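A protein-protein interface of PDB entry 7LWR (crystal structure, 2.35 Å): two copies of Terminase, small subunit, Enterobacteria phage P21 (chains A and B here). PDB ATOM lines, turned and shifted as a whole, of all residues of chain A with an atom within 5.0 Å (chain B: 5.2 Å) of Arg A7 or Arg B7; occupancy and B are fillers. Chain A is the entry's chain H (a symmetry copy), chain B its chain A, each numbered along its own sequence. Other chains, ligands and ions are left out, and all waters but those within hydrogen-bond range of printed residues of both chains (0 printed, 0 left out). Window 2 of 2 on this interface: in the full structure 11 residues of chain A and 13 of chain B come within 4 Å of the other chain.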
ATOM      1  N   MET A   1      20.198 -16.369  16.371  1.00  0.00           N
ATOM      2  CA  MET A   1      20.066 -17.781  16.759  1.00  0.00           C
ATOM      3  C   MET A   1      20.786 -18.681  15.751  1.00  0.00           C
ATOM      4  O   MET A   1      20.948 -18.287  14.606  1.00  0.00           O
ATOM      5  CB  MET A   1      18.599 -18.194  16.827  1.00  0.00           C
ATOM      6  CG  MET A   1      17.892 -18.097  15.503  1.00  0.00           C
ATOM      7  SD  MET A   1      16.191 -18.658  15.515  1.00  0.00           S
ATOM      8  CE  MET A   1      16.337 -20.203  16.400  1.00  0.00           C
ATOM      9  N   VAL A   3      20.987 -21.588  13.151  1.00  0.00           N
ATOM     10  CA  VAL A   3      20.185 -22.291  12.116  1.00  0.00           C
ATOM     11  C   VAL A   3      21.119 -22.974  11.120  1.00  0.00           C
ATOM     12  O   VAL A   3      22.281 -22.593  11.012  1.00  0.00           O
ATOM     13  CB  VAL A   3      19.216 -21.342  11.400  1.00  0.00           C
ATOM     14  CG1 VAL A   3      18.252 -20.695  12.358  1.00  0.00           C
ATOM     15  CG2 VAL A   3      19.941 -20.303  10.571  1.00  0.00           C
ATOM     16  N   ASN A   4      20.560 -23.918  10.365  1.00  0.00           N
ATOM     17  CA  ASN A   4      21.232 -24.601   9.226  1.00  0.00           C
ATOM     18  C   ASN A   4      20.969 -23.773   7.953  1.00  0.00           C
ATOM     19  O   ASN A   4      20.227 -22.822   8.018  1.00  0.00           O
ATOM     20  CB  ASN A   4      20.890 -26.103   9.200  1.00  0.00           C
ATOM     21  CG  ASN A   4      19.452 -26.438   8.823  1.00  0.00           C
ATOM     22  OD1 ASN A   4      18.765 -25.636   8.204  1.00  0.00           O
ATOM     23  ND2 ASN A   4      19.011 -27.652   9.135  1.00  0.00           N
ATOM     24  N   LYS A   5      21.623 -24.123   6.847  1.00  0.00           N
ATOM     25  CA  LYS A   5      21.504 -23.466   5.523  1.00  0.00           C
ATOM     26  C   LYS A   5      20.062 -23.381   5.039  1.00  0.00           C
ATOM     27  O   LYS A   5      19.680 -22.370   4.528  1.00  0.00           O
ATOM     28  CB  LYS A   5      22.333 -24.248   4.511  1.00  0.00           C
ATOM     29  CG  LYS A   5      22.436 -23.676   3.119  1.00  0.00           C
ATOM     30  CD  LYS A   5      23.446 -24.382   2.284  1.00  0.00           C
ATOM     31  CE  LYS A   5      24.857 -23.922   2.583  1.00  0.00           C
ATOM     32  NZ  LYS A   5      25.859 -24.763   1.893  1.00  0.00           N
ATOM     33  N   LYS A   6      19.317 -24.467   5.135  1.00  0.00           N
ATOM     34  CA  LYS A   6      17.899 -24.498   4.737  1.00  0.00           C
ATOM     35  C   LYS A   6      17.132 -23.406   5.483  1.00  0.00           C
ATOM     36  O   LYS A   6      16.417 -22.610   4.817  1.00  0.00           O
ATOM     37  CB  LYS A   6      17.341 -25.893   4.942  1.00  0.00           C
ATOM     38  CG  LYS A   6      15.835 -26.021   5.082  1.00  0.00           C
ATOM     39  CD  LYS A   6      15.411 -27.474   5.097  1.00  0.00           C
ATOM     40  CE  LYS A   6      13.946 -27.683   5.379  1.00  0.00           C
ATOM     41  NZ  LYS A   6      13.565 -29.098   5.193  1.00  0.00           N
ATOM     42  N   ARG A   7      17.215 -23.396   6.803  1.00  0.00           N
ATOM     43  CA  ARG A   7      16.446 -22.416   7.595  1.00  0.00           C
ATOM     44  C   ARG A   7      16.931 -21.027   7.238  1.00  0.00           C
ATOM     45  O   ARG A   7      16.124 -20.141   7.149  1.00  0.00           O
ATOM     46  CB  ARG A   7      16.575 -22.631   9.100  1.00  0.00           C
ATOM     47  CG  ARG A   7      15.823 -21.607   9.934  1.00  0.00           C
ATOM     48  CD  ARG A   7      14.331 -21.520   9.667  1.00  0.00           C
ATOM     49  NE  ARG A   7      13.669 -22.787   9.839  1.00  0.00           N
ATOM     50  CZ  ARG A   7      13.120 -23.224  10.955  1.00  0.00           C
ATOM     51  NH1 ARG A   7      13.144 -22.489  12.055  1.00  0.00           N
ATOM     52  NH2 ARG A   7      12.559 -24.422  10.972  1.00  0.00           N
ATOM     53  N   LEU A   8      18.243 -20.866   7.141  1.00  0.00           N
ATOM     54  CA  LEU A   8      18.867 -19.565   6.830  1.00  0.00           C
ATOM     55  C   LEU A   8      18.356 -19.030   5.503  1.00  0.00           C
ATOM     56  O   LEU A   8      18.069 -17.834   5.440  1.00  0.00           O
ATOM     57  CB  LEU A   8      20.384 -19.688   6.772  1.00  0.00           C
ATOM     58  CG  LEU A   8      21.053 -18.336   6.803  1.00  0.00           C
ATOM     59  CD1 LEU A   8      20.751 -17.661   8.132  1.00  0.00           C
ATOM     60  CD2 LEU A   8      22.532 -18.452   6.533  1.00  0.00           C
ATOM     61  N   ALA A   9      18.367 -19.872   4.472  1.00  0.00           N
ATOM     62  CA  ALA A   9      17.793 -19.534   3.158  1.00  0.00           C
ATOM     63  C   ALA A   9      16.303 -19.181   3.291  1.00  0.00           C
ATOM     64  O   ALA A   9      15.852 -18.211   2.660  1.00  0.00           O
ATOM     65  CB  ALA A   9      18.054 -20.658   2.214  1.00  0.00           C
ATOM     66  N   GLU A  10      15.579 -19.913   4.135  1.00  0.00           N
ATOM     67  CA  GLU A  10      14.128 -19.688   4.346  1.00  0.00           C
ATOM     68  C   GLU A  10      13.933 -18.334   5.049  1.00  0.00           C
ATOM     69  O   GLU A  10      12.963 -17.641   4.767  1.00  0.00           O
ATOM     70  CB  GLU A  10      13.497 -20.878   5.062  1.00  0.00           C
ATOM     71  CG  GLU A  10      11.970 -20.800   5.148  1.00  0.00           C
ATOM     72  CD  GLU A  10      11.257 -21.936   5.881  1.00  0.00           C
ATOM     73  OE1 GLU A  10      10.019 -22.051   5.706  1.00  0.00           O
ATOM     74  OE2 GLU A  10      11.921 -22.654   6.651  1.00  0.00           O
ATOM     75  N   ILE A  11      14.849 -17.944   5.919  1.00  0.00           N
ATOM     76  CA  ILE A  11      14.783 -16.660   6.655  1.00  0.00           C
ATOM     77  C   ILE A  11      15.034 -15.512   5.670  1.00  0.00           C
ATOM     78  O   ILE A  11      14.277 -14.524   5.743  1.00  0.00           O
ATOM     79  CB  ILE A  11      15.699 -16.689   7.886  1.00  0.00           C
ATOM     80  CG1 ILE A  11      15.206 -17.730   8.892  1.00  0.00           C
ATOM     81  CG2 ILE A  11      15.827 -15.328   8.537  1.00  0.00           C
ATOM     82  CD1 ILE A  11      16.235 -18.103   9.920  1.00  0.00           C
ATOM     83  N   MET B   1      10.250 -15.852   5.565  1.00  0.00           N
ATOM     84  CA  MET B   1       9.190 -16.694   6.099  1.00  0.00           C
ATOM     85  C   MET B   1       8.385 -15.921   7.164  1.00  0.00           C
ATOM     86  O   MET B   1       8.946 -15.006   7.818  1.00  0.00           O
ATOM     87  CB  MET B   1       9.774 -17.979   6.683  1.00  0.00           C
ATOM     88  CG  MET B   1      10.862 -17.678   7.701  1.00  0.00           C
ATOM     89  SD  MET B   1      11.726 -19.096   8.331  1.00  0.00           S
ATOM     90  CE  MET B   1      10.423 -19.957   9.208  1.00  0.00           C
ATOM     91  N   VAL B   3       6.889 -15.238  10.657  1.00  0.00           N
ATOM     92  CA  VAL B   3       7.233 -15.480  12.080  1.00  0.00           C
ATOM     93  C   VAL B   3       6.509 -14.492  12.999  1.00  0.00           C
ATOM     94  O   VAL B   3       6.125 -13.401  12.558  1.00  0.00           O
ATOM     95  CB  VAL B   3       8.744 -15.417  12.343  1.00  0.00           C
ATOM     96  CG1 VAL B   3       9.526 -16.428  11.532  1.00  0.00           C
ATOM     97  CG2 VAL B   3       9.301 -14.028  12.147  1.00  0.00           C
ATOM     98  N   ASN B   4       6.417 -14.898  14.274  1.00  0.00           N
ATOM     99  CA  ASN B   4       5.905 -14.086  15.404  1.00  0.00           C
ATOM    100  C   ASN B   4       7.016 -13.203  15.967  1.00  0.00           C
ATOM    101  O   ASN B   4       8.163 -13.399  15.605  1.00  0.00           O
ATOM    102  CB  ASN B   4       5.261 -14.965  16.460  1.00  0.00           C
ATOM    103  CG  ASN B   4       6.199 -15.860  17.253  1.00  0.00           C
ATOM    104  OD1 ASN B   4       7.415 -15.670  17.285  1.00  0.00           O
ATOM    105  ND2 ASN B   4       5.601 -16.867  17.888  1.00  0.00           N
ATOM    106  N   LYS B   5       6.648 -12.250  16.821  1.00  0.00           N
ATOM    107  CA  LYS B   5       7.562 -11.223  17.400  1.00  0.00           C
ATOM    108  C   LYS B   5       8.710 -11.929  18.127  1.00  0.00           C
ATOM    109  O   LYS B   5       9.856 -11.522  17.904  1.00  0.00           O
ATOM    110  CB  LYS B   5       6.805 -10.249  18.296  1.00  0.00           C
ATOM    111  CG  LYS B   5       7.660  -9.342  19.169  1.00  0.00           C
ATOM    112  CD  LYS B   5       6.986  -8.055  19.580  1.00  0.00           C
ATOM    113  CE  LYS B   5       5.527  -8.259  19.948  1.00  0.00           C
ATOM    114  NZ  LYS B   5       4.658  -7.133  19.540  1.00  0.00           N
ATOM    115  N   LYS B   6       8.401 -12.994  18.877  1.00  0.00           N
ATOM    116  CA  LYS B   6       9.384 -13.784  19.647  1.00  0.00           C
ATOM    117  C   LYS B   6      10.434 -14.366  18.684  1.00  0.00           C
ATOM    118  O   LYS B   6      11.633 -14.123  18.917  1.00  0.00           O
ATOM    119  CB  LYS B   6       8.691 -14.827  20.528  1.00  0.00           C
ATOM    120  CG  LYS B   6       9.654 -15.703  21.334  1.00  0.00           C
ATOM    121  CD  LYS B   6       9.331 -15.850  22.813  1.00  0.00           C
ATOM    122  CE  LYS B   6       9.715 -17.203  23.385  1.00  0.00           C
ATOM    123  NZ  LYS B   6       8.888 -18.287  22.813  1.00  0.00           N
ATOM    124  N   ARG B   7      10.016 -15.055  17.629  1.00  0.00           N
ATOM    125  CA  ARG B   7      10.932 -15.707  16.660  1.00  0.00           C
ATOM    126  C   ARG B   7      11.813 -14.673  15.956  1.00  0.00           C
ATOM    127  O   ARG B   7      13.029 -14.911  15.813  1.00  0.00           O
ATOM    128  CB  ARG B   7      10.180 -16.593  15.672  1.00  0.00           C
ATOM    129  CG  ARG B   7      11.058 -17.284  14.623  1.00  0.00           C
ATOM    130  CD  ARG B   7      12.185 -18.068  15.267  1.00  0.00           C
ATOM    131  NE  ARG B   7      11.646 -19.076  16.127  1.00  0.00           N
ATOM    132  CZ  ARG B   7      11.192 -20.242  15.709  1.00  0.00           C
ATOM    133  NH1 ARG B   7      11.250 -20.586  14.434  1.00  0.00           N
ATOM    134  NH2 ARG B   7      10.688 -21.093  16.579  1.00  0.00           N
ATOM    135  N   LEU B   8      11.221 -13.554  15.547  1.00  0.00           N
ATOM    136  CA  LEU B   8      11.936 -12.488  14.802  1.00  0.00           C
ATOM    137  C   LEU B   8      13.006 -11.904  15.713  1.00  0.00           C
ATOM    138  O   LEU B   8      14.114 -11.671  15.250  1.00  0.00           O
ATOM    139  CB  LEU B   8      10.942 -11.436  14.318  1.00  0.00           C
ATOM    140  CG  LEU B   8      11.511 -10.281  13.511  1.00  0.00           C
ATOM    141  CD1 LEU B   8      11.997 -10.738  12.184  1.00  0.00           C
ATOM    142  CD2 LEU B   8      10.451  -9.250  13.294  1.00  0.00           C
ATOM    143  N   ALA B   9      12.664 -11.719  16.986  1.00  0.00           N
ATOM    144  CA  ALA B   9      13.560 -11.182  18.019  1.00  0.00           C
ATOM    145  C   ALA B   9      14.738 -12.141  18.225  1.00  0.00           C
ATOM    146  O   ALA B   9      15.864 -11.667  18.341  1.00  0.00           O
ATOM    147  CB  ALA B   9      12.765 -10.911  19.255  1.00  0.00           C
ATOM    148  N   GLU B  10      14.487 -13.447  18.205  1.00  0.00           N
ATOM    149  CA  GLU B  10      15.540 -14.490  18.322  1.00  0.00           C
ATOM    150  C   GLU B  10      16.452 -14.458  17.083  1.00  0.00           C
ATOM    151  O   GLU B  10      17.657 -14.640  17.232  1.00  0.00           O
ATOM    152  CB  GLU B  10      14.941 -15.876  18.530  1.00  0.00           C
ATOM    153  CG  GLU B  10      16.017 -16.937  18.721  1.00  0.00           C
ATOM    154  CD  GLU B  10      15.605 -18.236  19.400  1.00  0.00           C
ATOM    155  OE1 GLU B  10      14.427 -18.600  19.300  1.00  0.00           O
ATOM    156  OE2 GLU B  10      16.478 -18.881  19.999  1.00  0.00           O
ATOM    157  N   ILE B  11      15.909 -14.170  15.902  1.00  0.00           N
ATOM    158  CA  ILE B  11      16.689 -14.111  14.635  1.00  0.00           C
ATOM    159  C   ILE B  11      17.662 -12.924  14.678  1.00  0.00           C
ATOM    160  O   ILE B  11      18.871 -13.112  14.421  1.00  0.00           O
ATOM    161  CB  ILE B  11      15.730 -14.069  13.452  1.00  0.00           C
ATOM    162  CG1 ILE B  11      14.978 -15.396  13.329  1.00  0.00           C
ATOM    163  CG2 ILE B  11      16.470 -13.691  12.176  1.00  0.00           C
ATOM    164  CD1 ILE B  11      13.827 -15.380  12.389  1.00  0.00           C
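Among the printed residues, pairs that only touch across the chains: Arg A7 with Met B1, Arg A7 with Arg B7 and Ile A11 with Met B1.
OD1 of Asn B4 is in hydrogen-bond range of N of Arg B7, 2.7 Å away. The side-chain amide oxygen (OD1) of Asn A4 lies within hydrogen-bond range of the backbone NH (N) of Arg A7 (3.1 Å). NE of Arg A7 lies within salt-bridge range of OE2 of Glu A10, 3.6 Å away.
O of Glu A10 is in hydrogen-bond range of N of Met B1 (3.3 Å). O of Glu B10 sits at hydrogen-bond distance from N of Met A1 (3.2 Å).
Arg A7 touches just these residues of chain B: Met B1 (3.8 Å) and Arg B7 (3.6 Å). Of chain A, only Arg A7 (3.6 Å) comes within 4 Å of Arg B7. Printed residues of chain B within 4 Å of Met A1: Glu B10. Printed residues of chain A within 4 Å of Met B1: Arg A7 (3.8 Å), Glu A10 (3.3 Å) and Ile A11 (3.8 Å). Printed residues of chain B within 4 Å of Glu A10: Met B1 (3.3 Å). Of the printed residues of chain A, Glu B10 touches Met A1 (3.2 Å). Of the printed residues of chain B, Ile A11 touches Met B1. Lys A5 touches none of the printed residues of chain B. The nearest printed residue of chain B that does not touch Arg A7 is Ile B11 (6.7 Å). The nearest printed residue of chain B that does not touch Met A1 is Ile B11 (4.02 Å).
Of the 10 printed residues of chain A, 4 touch a printed residue of chain B. Hydrophobic or aromatic side chains of chain A within 4 Å of the printed part of chain B: Met A1 and Ile A11. Hydrophobic or aromatic side chains of chain B within 4 Å of the printed part of chain A: Met B1.
Met A1 touches Glu B10, and with the chains exchanged Glu A10 touches Met B1. Arg A7 touches Met B1, but with the chains exchanged Met A1 does not touch Arg B7 (4.1 Å). Arg A7 touches its own counterpart, Arg B7. Ile A11 touches Met B1, but with the chains exchanged Met A1 does not touch Ile B11 (4.02 Å). 10 positions are printed for both chains. Of the 5 pairs that touch across the chains among the printed residues, 3 have their exchanged pair printed and touching as well.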
